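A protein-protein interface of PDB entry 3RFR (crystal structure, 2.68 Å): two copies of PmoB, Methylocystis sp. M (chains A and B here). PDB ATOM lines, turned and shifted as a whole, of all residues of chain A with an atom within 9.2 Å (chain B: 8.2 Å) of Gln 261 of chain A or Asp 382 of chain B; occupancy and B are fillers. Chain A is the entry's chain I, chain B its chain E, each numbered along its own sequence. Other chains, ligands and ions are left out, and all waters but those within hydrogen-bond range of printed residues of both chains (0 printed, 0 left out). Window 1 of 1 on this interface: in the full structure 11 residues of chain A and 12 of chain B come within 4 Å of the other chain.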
ATOM      1  N   PRO A 107      -0.682 -11.854  23.934  1.00  0.00           N
ATOM      2  CA  PRO A 107      -1.336 -11.421  22.688  1.00  0.00           C
ATOM      3  C   PRO A 107      -0.568 -11.866  21.459  1.00  0.00           C
ATOM      4  O   PRO A 107      -1.070 -11.772  20.322  1.00  0.00           O
ATOM      5  CB  PRO A 107      -1.321  -9.919  22.783  1.00  0.00           C
ATOM      6  CG  PRO A 107      -0.214  -9.604  23.725  1.00  0.00           C
ATOM      7  CD  PRO A 107       0.023 -10.752  24.617  1.00  0.00           C
ATOM      8  N   ARG A 108       0.646 -12.345  21.685  1.00  0.00           N
ATOM      9  CA  ARG A 108       1.522 -12.785  20.609  1.00  0.00           C
ATOM     10  C   ARG A 108       1.797 -14.256  20.807  1.00  0.00           C
ATOM     11  O   ARG A 108       1.166 -14.897  21.697  1.00  0.00           O
ATOM     12  CB  ARG A 108       2.809 -11.968  20.542  1.00  0.00           C
ATOM     13  CG  ARG A 108       2.526 -10.521  20.673  1.00  0.00           C
ATOM     14  CD  ARG A 108       3.384  -9.654  19.786  1.00  0.00           C
ATOM     15  NE  ARG A 108       4.821  -9.707  20.124  1.00  0.00           N
ATOM     16  CZ  ARG A 108       5.446  -8.897  20.955  1.00  0.00           C
ATOM     17  NH1 ARG A 108       4.798  -7.931  21.558  1.00  0.00           N
ATOM     18  NH2 ARG A 108       6.734  -9.067  21.164  1.00  0.00           N
ATOM     19  N   SER A 109       2.678 -14.834  19.978  1.00  0.00           N
ATOM     20  CA  SER A 109       2.780 -16.304  20.035  1.00  0.00           C
ATOM     21  C   SER A 109       3.824 -16.741  21.083  1.00  0.00           C
ATOM     22  O   SER A 109       4.762 -15.930  21.403  1.00  0.00           O
ATOM     23  CB  SER A 109       3.003 -16.901  18.672  1.00  0.00           C
ATOM     24  OG  SER A 109       4.201 -16.406  18.205  1.00  0.00           O
ATOM     25  N   THR A 257       2.952   7.623  16.477  1.00  0.00           N
ATOM     26  CA  THR A 257       2.420   6.332  16.096  1.00  0.00           C
ATOM     27  C   THR A 257       3.490   5.238  16.176  1.00  0.00           C
ATOM     28  O   THR A 257       4.675   5.513  15.945  1.00  0.00           O
ATOM     29  CB  THR A 257       1.708   6.344  14.700  1.00  0.00           C
ATOM     30  OG1 THR A 257       2.653   6.592  13.674  1.00  0.00           O
ATOM     31  CG2 THR A 257       0.603   7.415  14.621  1.00  0.00           C
ATOM     32  N   ILE A 258       3.053   4.014  16.550  1.00  0.00           N
ATOM     33  CA  ILE A 258       3.947   2.858  16.614  1.00  0.00           C
ATOM     34  C   ILE A 258       3.612   1.863  15.516  1.00  0.00           C
ATOM     35  O   ILE A 258       2.482   1.832  15.030  1.00  0.00           O
ATOM     36  CB  ILE A 258       3.950   2.185  17.987  1.00  0.00           C
ATOM     37  CG1 ILE A 258       2.561   1.608  18.320  1.00  0.00           C
ATOM     38  CG2 ILE A 258       4.358   3.180  19.043  1.00  0.00           C
ATOM     39  CD1 ILE A 258       2.474   0.756  19.558  1.00  0.00           C
ATOM     40  N   PRO A 259       4.617   1.120  15.024  1.00  0.00           N
ATOM     41  CA  PRO A 259       4.329   0.002  14.103  1.00  0.00           C
ATOM     42  C   PRO A 259       3.739  -1.240  14.833  1.00  0.00           C
ATOM     43  O   PRO A 259       3.959  -1.368  16.010  1.00  0.00           O
ATOM     44  CB  PRO A 259       5.723  -0.277  13.492  1.00  0.00           C
ATOM     45  CG  PRO A 259       6.670   0.221  14.493  1.00  0.00           C
ATOM     46  CD  PRO A 259       6.051   1.470  14.997  1.00  0.00           C
ATOM     47  N   LEU A 260       2.997  -2.113  14.145  1.00  0.00           N
ATOM     48  CA  LEU A 260       2.377  -3.305  14.814  1.00  0.00           C
ATOM     49  C   LEU A 260       3.417  -4.036  15.657  1.00  0.00           C
ATOM     50  O   LEU A 260       4.587  -4.136  15.272  1.00  0.00           O
ATOM     51  CB  LEU A 260       1.812  -4.338  13.823  1.00  0.00           C
ATOM     52  CG  LEU A 260       0.902  -3.878  12.681  1.00  0.00           C
ATOM     53  CD1 LEU A 260       0.813  -4.959  11.581  1.00  0.00           C
ATOM     54  CD2 LEU A 260      -0.427  -3.434  13.184  1.00  0.00           C
ATOM     55  N   GLN A 261       3.030  -4.522  16.813  1.00  0.00           N
ATOM     56  CA  GLN A 261       3.987  -5.112  17.692  1.00  0.00           C
ATOM     57  C   GLN A 261       3.877  -6.634  17.537  1.00  0.00           C
ATOM     58  O   GLN A 261       2.857  -7.228  17.938  1.00  0.00           O
ATOM     59  CB  GLN A 261       3.599  -4.696  19.101  1.00  0.00           C
ATOM     60  CG  GLN A 261       3.673  -3.217  19.307  1.00  0.00           C
ATOM     61  CD  GLN A 261       5.082  -2.752  19.414  1.00  0.00           C
ATOM     62  OE1 GLN A 261       5.571  -2.027  18.553  1.00  0.00           O
ATOM     63  NE2 GLN A 261       5.779  -3.191  20.475  1.00  0.00           N
ATOM     64  N   ALA A 262       4.892  -7.271  16.946  1.00  0.00           N
ATOM     65  CA  ALA A 262       4.831  -8.738  16.670  1.00  0.00           C
ATOM     66  C   ALA A 262       6.127  -9.436  17.016  1.00  0.00           C
ATOM     67  O   ALA A 262       7.240  -8.780  17.073  1.00  0.00           O
ATOM     68  CB  ALA A 262       4.479  -9.017  15.244  1.00  0.00           C
ATOM     69  N   GLY A 263       6.007 -10.746  17.231  1.00  0.00           N
ATOM     70  CA  GLY A 263       7.155 -11.556  17.608  1.00  0.00           C
ATOM     71  C   GLY A 263       6.795 -12.445  18.779  1.00  0.00           C
ATOM     72  O   GLY A 263       6.100 -12.001  19.675  1.00  0.00           O
ATOM     73  N   LEU A 264       7.238 -13.702  18.718  1.00  0.00           N
ATOM     74  CA  LEU A 264       7.347 -14.641  19.815  1.00  0.00           C
ATOM     75  C   LEU A 264       7.734 -14.006  21.138  1.00  0.00           C
ATOM     76  O   LEU A 264       8.495 -13.008  21.178  1.00  0.00           O
ATOM     77  CB  LEU A 264       8.431 -15.664  19.451  1.00  0.00           C
ATOM     78  CG  LEU A 264       8.574 -17.007  20.162  1.00  0.00           C
ATOM     79  CD1 LEU A 264       7.252 -17.880  20.253  1.00  0.00           C
ATOM     80  CD2 LEU A 264       9.725 -17.739  19.439  1.00  0.00           C
ATOM     81  N   GLN A 265       7.233 -14.585  22.233  1.00  0.00           N
ATOM     82  CA  GLN A 265       7.475 -13.994  23.551  1.00  0.00           C
ATOM     83  C   GLN A 265       8.517 -14.785  24.308  1.00  0.00           C
ATOM     84  O   GLN A 265       8.687 -15.957  24.037  1.00  0.00           O
ATOM     85  CB  GLN A 265       6.178 -13.898  24.333  1.00  0.00           C
ATOM     86  CG  GLN A 265       5.109 -13.210  23.558  1.00  0.00           C
ATOM     87  CD  GLN A 265       3.893 -12.790  24.396  1.00  0.00           C
ATOM     88  OE1 GLN A 265       3.275 -13.600  25.173  1.00  0.00           O
ATOM     89  NE2 GLN A 265       3.533 -11.493  24.235  1.00  0.00           N
ATOM     90  N   SER B  33      22.684   2.874  13.696  1.00  0.00           N
ATOM     91  CA  SER B  33      21.500   2.794  12.861  1.00  0.00           C
ATOM     92  C   SER B  33      20.765   1.438  12.891  1.00  0.00           C
ATOM     93  O   SER B  33      19.721   1.295  12.271  1.00  0.00           O
ATOM     94  CB  SER B  33      21.829   3.200  11.435  1.00  0.00           C
ATOM     95  OG  SER B  33      22.721   2.275  10.859  1.00  0.00           O
ATOM     96  N   GLN B  34      21.280   0.462  13.632  1.00  0.00           N
ATOM     97  CA  GLN B  34      20.522  -0.765  13.837  1.00  0.00           C
ATOM     98  C   GLN B  34      19.452  -0.584  14.893  1.00  0.00           C
ATOM     99  O   GLN B  34      19.552   0.296  15.732  1.00  0.00           O
ATOM    100  CB  GLN B  34      21.437  -1.925  14.217  1.00  0.00           C
ATOM    101  CG  GLN B  34      22.421  -2.279  13.163  1.00  0.00           C
ATOM    102  CD  GLN B  34      23.354  -3.323  13.617  1.00  0.00           C
ATOM    103  OE1 GLN B  34      24.105  -3.126  14.566  1.00  0.00           O
ATOM    104  NE2 GLN B  34      23.340  -4.444  12.955  1.00  0.00           N
ATOM    105  N   GLN B  35      18.444  -1.453  14.849  1.00  0.00           N
ATOM    106  CA  GLN B  35      17.288  -1.366  15.727  1.00  0.00           C
ATOM    107  C   GLN B  35      17.681  -1.650  17.158  1.00  0.00           C
ATOM    108  O   GLN B  35      18.412  -2.585  17.436  1.00  0.00           O
ATOM    109  CB  GLN B  35      16.152  -2.281  15.288  1.00  0.00           C
ATOM    110  CG  GLN B  35      15.373  -1.722  14.129  1.00  0.00           C
ATOM    111  CD  GLN B  35      14.293  -2.653  13.647  1.00  0.00           C
ATOM    112  OE1 GLN B  35      14.566  -3.670  13.015  1.00  0.00           O
ATOM    113  NE2 GLN B  35      13.054  -2.300  13.918  1.00  0.00           N
ATOM    114  N   ALA B  36      17.170  -0.813  18.054  1.00  0.00           N
ATOM    115  CA  ALA B  36      17.595  -0.755  19.413  1.00  0.00           C
ATOM    116  C   ALA B  36      17.259  -2.032  20.103  1.00  0.00           C
ATOM    117  O   ALA B  36      18.094  -2.536  20.856  1.00  0.00           O
ATOM    118  CB  ALA B  36      16.914   0.384  20.097  1.00  0.00           C
ATOM    119  N   PHE B  37      16.051  -2.564  19.877  1.00  0.00           N
ATOM    120  CA  PHE B  37      15.665  -3.756  20.607  1.00  0.00           C
ATOM    121  C   PHE B  37      16.562  -4.924  20.220  1.00  0.00           C
ATOM    122  O   PHE B  37      17.016  -5.686  21.065  1.00  0.00           O
ATOM    123  CB  PHE B  37      14.171  -4.041  20.500  1.00  0.00           C
ATOM    124  CG  PHE B  37      13.755  -4.800  19.273  1.00  0.00           C
ATOM    125  CD1 PHE B  37      13.521  -4.138  18.064  1.00  0.00           C
ATOM    126  CD2 PHE B  37      13.528  -6.170  19.338  1.00  0.00           C
ATOM    127  CE1 PHE B  37      13.100  -4.837  16.921  1.00  0.00           C
ATOM    128  CE2 PHE B  37      13.129  -6.871  18.215  1.00  0.00           C
ATOM    129  CZ  PHE B  37      12.912  -6.199  16.992  1.00  0.00           C
ATOM    130  N   LEU B  38      16.901  -5.031  18.946  1.00  0.00           N
ATOM    131  CA  LEU B  38      17.798  -6.091  18.544  1.00  0.00           C
ATOM    132  C   LEU B  38      19.162  -5.893  19.170  1.00  0.00           C
ATOM    133  O   LEU B  38      19.775  -6.843  19.620  1.00  0.00           O
ATOM    134  CB  LEU B  38      17.875  -6.209  17.031  1.00  0.00           C
ATOM    135  CG  LEU B  38      16.555  -6.681  16.409  1.00  0.00           C
ATOM    136  CD1 LEU B  38      16.688  -6.751  14.918  1.00  0.00           C
ATOM    137  CD2 LEU B  38      16.070  -8.020  16.994  1.00  0.00           C
ATOM    138  N   ARG B  39      19.651  -4.667  19.212  1.00  0.00           N
ATOM    139  CA  ARG B  39      20.951  -4.437  19.789  1.00  0.00           C
ATOM    140  C   ARG B  39      20.952  -4.752  21.271  1.00  0.00           C
ATOM    141  O   ARG B  39      21.921  -5.228  21.814  1.00  0.00           O
ATOM    142  CB  ARG B  39      21.359  -3.009  19.589  1.00  0.00           C
ATOM    143  CG  ARG B  39      21.880  -2.686  18.240  1.00  0.00           C
ATOM    144  CD  ARG B  39      22.499  -1.334  18.310  1.00  0.00           C
ATOM    145  NE  ARG B  39      21.547  -0.287  17.983  1.00  0.00           N
ATOM    146  CZ  ARG B  39      21.543   0.928  18.529  1.00  0.00           C
ATOM    147  NH1 ARG B  39      20.644   1.827  18.146  1.00  0.00           N
ATOM    148  NH2 ARG B  39      22.418   1.244  19.457  1.00  0.00           N
ATOM    149  N   MET B  40      19.845  -4.497  21.936  1.00  0.00           N
ATOM    150  CA  MET B  40      19.751  -4.784  23.356  1.00  0.00           C
ATOM    151  C   MET B  40      19.525  -6.263  23.674  1.00  0.00           C
ATOM    152  O   MET B  40      20.039  -6.760  24.675  1.00  0.00           O
ATOM    153  CB  MET B  40      18.672  -3.914  24.002  1.00  0.00           C
ATOM    154  CG  MET B  40      19.065  -2.463  24.076  1.00  0.00           C
ATOM    155  SD  MET B  40      17.731  -1.445  24.679  1.00  0.00           S
ATOM    156  CE  MET B  40      17.954  -1.859  26.370  1.00  0.00           C
ATOM    157  N   TYR B 293      10.196   5.138  28.952  1.00  0.00           N
ATOM    158  CA  TYR B 293      11.233   5.885  28.295  1.00  0.00           C
ATOM    159  C   TYR B 293      10.583   7.029  27.555  1.00  0.00           C
ATOM    160  O   TYR B 293       9.566   6.855  26.884  1.00  0.00           O
ATOM    161  CB  TYR B 293      12.115   4.984  27.380  1.00  0.00           C
ATOM    162  CG  TYR B 293      11.424   4.374  26.176  1.00  0.00           C
ATOM    163  CD1 TYR B 293      10.571   3.282  26.324  1.00  0.00           C
ATOM    164  CD2 TYR B 293      11.616   4.893  24.895  1.00  0.00           C
ATOM    165  CE1 TYR B 293       9.927   2.734  25.257  1.00  0.00           C
ATOM    166  CE2 TYR B 293      10.964   4.335  23.801  1.00  0.00           C
ATOM    167  CZ  TYR B 293      10.119   3.255  24.005  1.00  0.00           C
ATOM    168  OH  TYR B 293       9.452   2.677  22.960  1.00  0.00           O
ATOM    169  N   ARG B 375      21.072   6.080  19.899  1.00  0.00           N
ATOM    170  CA  ARG B 375      19.753   5.871  19.331  1.00  0.00           C
ATOM    171  C   ARG B 375      18.980   4.732  19.982  1.00  0.00           C
ATOM    172  O   ARG B 375      18.158   4.084  19.354  1.00  0.00           O
ATOM    173  CB  ARG B 375      19.850   5.730  17.812  1.00  0.00           C
ATOM    174  CG  ARG B 375      20.200   7.001  17.082  1.00  0.00           C
ATOM    175  CD  ARG B 375      20.007   6.874  15.574  1.00  0.00           C
ATOM    176  NE  ARG B 375      18.624   6.538  15.167  1.00  0.00           N
ATOM    177  CZ  ARG B 375      18.169   5.304  14.868  1.00  0.00           C
ATOM    178  NH1 ARG B 375      18.962   4.219  14.922  1.00  0.00           N
ATOM    179  NH2 ARG B 375      16.895   5.145  14.512  1.00  0.00           N
ATOM    180  N   LEU B 376      19.252   4.474  21.250  1.00  0.00           N
ATOM    181  CA  LEU B 376      18.416   3.536  21.980  1.00  0.00           C
ATOM    182  C   LEU B 376      17.010   4.117  22.186  1.00  0.00           C
ATOM    183  O   LEU B 376      16.047   3.385  22.275  1.00  0.00           O
ATOM    184  CB  LEU B 376      19.065   3.123  23.292  1.00  0.00           C
ATOM    185  CG  LEU B 376      20.276   2.209  23.157  1.00  0.00           C
ATOM    186  CD1 LEU B 376      20.507   1.513  24.468  1.00  0.00           C
ATOM    187  CD2 LEU B 376      20.091   1.151  22.094  1.00  0.00           C
ATOM    188  N   SER B 377      16.901   5.443  22.208  1.00  0.00           N
ATOM    189  CA  SER B 377      15.610   6.153  22.266  1.00  0.00           C
ATOM    190  C   SER B 377      14.683   5.885  21.067  1.00  0.00           C
ATOM    191  O   SER B 377      13.469   6.092  21.156  1.00  0.00           O
ATOM    192  CB  SER B 377      15.872   7.656  22.346  1.00  0.00           C
ATOM    193  OG  SER B 377      16.675   8.064  21.245  1.00  0.00           O
ATOM    194  N   ASP B 378      15.263   5.458  19.951  1.00  0.00           N
ATOM    195  CA  ASP B 378      14.514   5.135  18.747  1.00  0.00           C
ATOM    196  C   ASP B 378      13.827   3.778  18.874  1.00  0.00           C
ATOM    197  O   ASP B 378      13.410   3.170  17.898  1.00  0.00           O
ATOM    198  CB  ASP B 378      15.427   5.208  17.513  1.00  0.00           C
ATOM    199  CG  ASP B 378      15.448   6.605  16.879  1.00  0.00           C
ATOM    200  OD1 ASP B 378      14.795   6.787  15.832  1.00  0.00           O
ATOM    201  OD2 ASP B 378      16.090   7.540  17.421  1.00  0.00           O
ATOM    202  N   LEU B 379      13.697   3.318  20.108  1.00  0.00           N
ATOM    203  CA  LEU B 379      13.000   2.080  20.421  1.00  0.00           C
ATOM    204  C   LEU B 379      11.541   2.113  20.016  1.00  0.00           C
ATOM    205  O   LEU B 379      10.961   1.083  19.717  1.00  0.00           O
ATOM    206  CB  LEU B 379      13.110   1.825  21.914  1.00  0.00           C
ATOM    207  CG  LEU B 379      12.677   0.495  22.502  1.00  0.00           C
ATOM    208  CD1 LEU B 379      13.386  -0.668  21.848  1.00  0.00           C
ATOM    209  CD2 LEU B 379      13.006   0.566  23.974  1.00  0.00           C
ATOM    210  N   ALA B 380      10.958   3.307  20.019  1.00  0.00           N
ATOM    211  CA  ALA B 380       9.527   3.493  19.735  1.00  0.00           C
ATOM    212  C   ALA B 380       9.200   3.283  18.252  1.00  0.00           C
ATOM    213  O   ALA B 380       8.043   3.170  17.884  1.00  0.00           O
ATOM    214  CB  ALA B 380       9.081   4.872  20.202  1.00  0.00           C
ATOM    215  N   TYR B 381      10.247   3.241  17.425  1.00  0.00           N
ATOM    216  CA  TYR B 381      10.161   3.018  15.990  1.00  0.00           C
ATOM    217  C   TYR B 381      10.231   1.520  15.685  1.00  0.00           C
ATOM    218  O   TYR B 381      10.007   1.120  14.563  1.00  0.00           O
ATOM    219  CB  TYR B 381      11.299   3.801  15.268  1.00  0.00           C
ATOM    220  CG  TYR B 381      11.355   3.570  13.765  1.00  0.00           C
ATOM    221  CD1 TYR B 381      10.550   4.310  12.901  1.00  0.00           C
ATOM    222  CD2 TYR B 381      12.199   2.578  13.202  1.00  0.00           C
ATOM    223  CE1 TYR B 381      10.577   4.070  11.503  1.00  0.00           C
ATOM    224  CE2 TYR B 381      12.218   2.326  11.805  1.00  0.00           C
ATOM    225  CZ  TYR B 381      11.406   3.077  10.972  1.00  0.00           C
ATOM    226  OH  TYR B 381      11.401   2.861   9.622  1.00  0.00           O
ATOM    227  N   ASP B 382      10.539   0.693  16.682  1.00  0.00           N
ATOM    228  CA  ASP B 382      10.730  -0.751  16.479  1.00  0.00           C
ATOM    229  C   ASP B 382       9.409  -1.480  16.621  1.00  0.00           C
ATOM    230  O   ASP B 382       8.409  -0.920  17.116  1.00  0.00           O
ATOM    231  CB  ASP B 382      11.744  -1.358  17.473  1.00  0.00           C
ATOM    232  CG  ASP B 382      13.150  -0.727  17.386  1.00  0.00           C
ATOM    233  OD1 ASP B 382      13.557  -0.173  16.334  1.00  0.00           O
ATOM    234  OD2 ASP B 382      13.876  -0.784  18.406  1.00  0.00           O
ATOM    235  N   THR B 383       9.420  -2.748  16.213  1.00  0.00           N
ATOM    236  CA  THR B 383       8.233  -3.589  16.268  1.00  0.00           C
ATOM    237  C   THR B 383       8.166  -4.372  17.545  1.00  0.00           C
ATOM    238  O   THR B 383       7.205  -5.096  17.774  1.00  0.00           O
ATOM    239  CB  THR B 383       8.119  -4.534  15.063  1.00  0.00           C
ATOM    240  OG1 THR B 383       9.430  -4.892  14.612  1.00  0.00           O
ATOM    241  CG2 THR B 383       7.361  -3.839  13.925  1.00  0.00           C
ATOM    242  N   ASP B 384       9.185  -4.231  18.377  1.00  0.00           N
ATOM    243  CA  ASP B 384       9.169  -4.804  19.701  1.00  0.00           C
ATOM    244  C   ASP B 384       9.735  -3.772  20.653  1.00  0.00           C
ATOM    245  O   ASP B 384      10.929  -3.564  20.665  1.00  0.00           O
ATOM    246  CB  ASP B 384       9.980  -6.085  19.755  1.00  0.00           C
ATOM    247  CG  ASP B 384       9.355  -7.129  20.676  1.00  0.00           C
ATOM    248  OD1 ASP B 384       8.272  -6.824  21.240  1.00  0.00           O
ATOM    249  OD2 ASP B 384       9.920  -8.248  20.841  1.00  0.00           O
ATOM    250  N   SER B 385       8.861  -3.088  21.399  1.00  0.00           N
ATOM    251  CA  SER B 385       9.255  -2.073  22.371  1.00  0.00           C
ATOM    252  C   SER B 385       9.601  -2.730  23.716  1.00  0.00           C
ATOM    253  O   SER B 385       8.777  -2.799  24.654  1.00  0.00           O
ATOM    254  CB  SER B 385       8.151  -1.023  22.523  1.00  0.00           C
ATOM    255  OG  SER B 385       8.434  -0.052  23.529  1.00  0.00           O
ATOM    256  N   GLN B 386      10.855  -3.179  23.790  1.00  0.00           N
ATOM    257  CA  GLN B 386      11.312  -4.060  24.825  1.00  0.00           C
ATOM    258  C   GLN B 386      12.803  -3.901  25.094  1.00  0.00           C
ATOM    259  O   GLN B 386      13.580  -3.955  24.156  1.00  0.00           O
ATOM    260  CB  GLN B 386      11.033  -5.449  24.343  1.00  0.00           C
ATOM    261  CG  GLN B 386      10.815  -6.429  25.423  1.00  0.00           C
ATOM    262  CD  GLN B 386       9.855  -7.503  25.025  1.00  0.00           C
ATOM    263  OE1 GLN B 386       9.163  -7.382  24.015  1.00  0.00           O
ATOM    264  NE2 GLN B 386       9.792  -8.572  25.833  1.00  0.00           N
ATOM    265  N   PRO B 408       9.125  -5.665  28.466  1.00  0.00           N
ATOM    266  CA  PRO B 408       8.343  -4.595  27.867  1.00  0.00           C
ATOM    267  C   PRO B 408       8.587  -3.251  28.532  1.00  0.00           C
ATOM    268  O   PRO B 408       8.640  -3.183  29.775  1.00  0.00           O
ATOM    269  CB  PRO B 408       6.904  -5.054  28.128  1.00  0.00           C
ATOM    270  CG  PRO B 408       6.963  -6.496  28.364  1.00  0.00           C
ATOM    271  CD  PRO B 408       8.247  -6.726  29.004  1.00  0.00           C
ATOM    272  N   VAL B 409       8.762  -2.196  27.738  1.00  0.00           N
ATOM    273  CA  VAL B 409       8.859  -0.821  28.290  1.00  0.00           C
ATOM    274  C   VAL B 409       8.019   0.117  27.468  1.00  0.00           C
ATOM    275  O   VAL B 409       7.928  -0.060  26.254  1.00  0.00           O
ATOM    276  CB  VAL B 409      10.291  -0.278  28.367  1.00  0.00           C
ATOM    277  CG1 VAL B 409      11.134  -1.055  29.416  1.00  0.00           C
ATOM    278  CG2 VAL B 409      10.935  -0.278  26.990  1.00  0.00           C
ATOM    279  N   PRO B 411       6.676   3.816  25.868  1.00  0.00           N
ATOM    280  CA  PRO B 411       7.171   5.163  25.562  1.00  0.00           C
ATOM    281  C   PRO B 411       6.269   6.258  26.135  1.00  0.00           C
ATOM    282  O   PRO B 411       5.057   6.099  26.185  1.00  0.00           O
ATOM    283  CB  PRO B 411       7.110   5.209  24.041  1.00  0.00           C
ATOM    284  CG  PRO B 411       6.037   4.258  23.665  1.00  0.00           C
ATOM    285  CD  PRO B 411       5.968   3.209  24.725  1.00  0.00           C
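The backbone carbonyl oxygen (O) of Asp 382 of chain B lies close to the side-chain amide oxygen (OE1) of Gln 261 of chain A (3.4 Å).
O of Thr 383 of chain B lies within hydrogen-bond range of N of Ala 262 of chain A.
OD1 of Asp 384 of chain B lies within salt-bridge range of NH2 of Arg 108 of chain A, 2.7 Å away.
The side-chain amide nitrogen of Gln 261 of chain A sits close to the backbone NH of Ser 385 of chain B, 3.2 Å away.
The side-chain carboxylate (OD2) of Asp 382 of chain B sits at hydrogen-bond distance from the backbone NH (N) of Phe 37 of chain B, 3.2 Å away.
The side-chain hydroxyl (OH) of Tyr 293 of chain B sits close to the backbone NH (N) of Ala 380 of chain B, 3.4 Å away.
The side-chain hydroxyl (OG) of Ser 385 of chain B sits at hydrogen-bond distance from the side-chain hydroxyl (OH) of Tyr 293 of chain B (3.0 Å).
OG of Ser 385 of chain B sits at hydrogen-bond distance from O of Val 409 of chain B (2.8 Å).
The backbone carbonyl oxygen of Gly 263 of chain A sits at hydrogen-bond distance from the guanidinium group of Arg 108 of chain A (2.7 Å).
The backbone carbonyl oxygen (O) of Pro 259 of chain A sits close to the side-chain amide oxygen (OE1) of Gln 261 of chain A (3.1 Å).
Among the printed residues, merely in contact across the chains: Ile 258 of chain A with Ala 380 of chain B (3.9 Å), Pro 259 of chain A with Ala 380 of chain B (3.9 Å), Pro 259 of chain A with Tyr 381 of chain B (3.5 Å), Pro 259 of chain A with Asp 382 of chain B (3.3 Å), Pro 259 of chain A with Thr 383 of chain B (3.9 Å), Leu 260 of chain A with Thr 383 of chain B (3.1 Å), Gln 261 of chain A with Thr 383 of chain B (3.2 Å) and Gln 261 of chain A with Asp 384 of chain B (3.8 Å).
Printed residues of chain B within 4 Å of Arg 108 of chain A: Asp 384 (2.7 Å).
Printed residues of chain B within 4 Å of Ile 258 of chain A: Ala 380.
Printed residues of chain B within 4 Å of Pro 259 of chain A: Ala 380, Tyr 381, Asp 382 and Thr 383.
Gln 261 of chain A touches just these residues of chain B: Asp 382, Thr 383, Asp 384 and Ser 385.
Of chain B, only Thr 383 comes within 4 Å of Ala 262 of chain A.
Of chain A, only Pro 259 and Gln 261 come within 4 Å of Asp 382 of chain B.
Thr 383 of chain B touches just these residues of chain A: Pro 259 (3.9 Å), Leu 260 (3.1 Å), Gln 261 (3.2 Å) and Ala 262 (3.3 Å).
Of the printed residues of chain A, Ser 385 of chain B touches Gln 261 (3.2 Å).
The nearest residue of chain B that does not touch Gln 261 of chain A is Ala 380 of chain B (5.8 Å).
The nearest residue of chain A that does not touch Asp 382 of chain B is Leu 260 of chain A (5.3 Å).
Printed residues of chain A that touch a printed residue of chain B: Arg 108, Ile 258, Pro 259, Leu 260, Gln 261 and Ala 262.
Of the 24 printed residues of chain B, 6 touch a printed residue of chain A.
Printed residues of chain B that touch a printed residue of chain A: Ala 380, Tyr 381, Asp 382, Thr 383, Asp 384 and Ser 385.
Among the printed residues, 12 pairs touch across the chains.
Among the printed residues, Asp or Glu carboxylates within 4 Å of a Lys or Arg side-chain nitrogen of the other chain: Arg 108 of chain A with Asp 384 of chain B (2.7 Å).
No position is printed for both chains.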
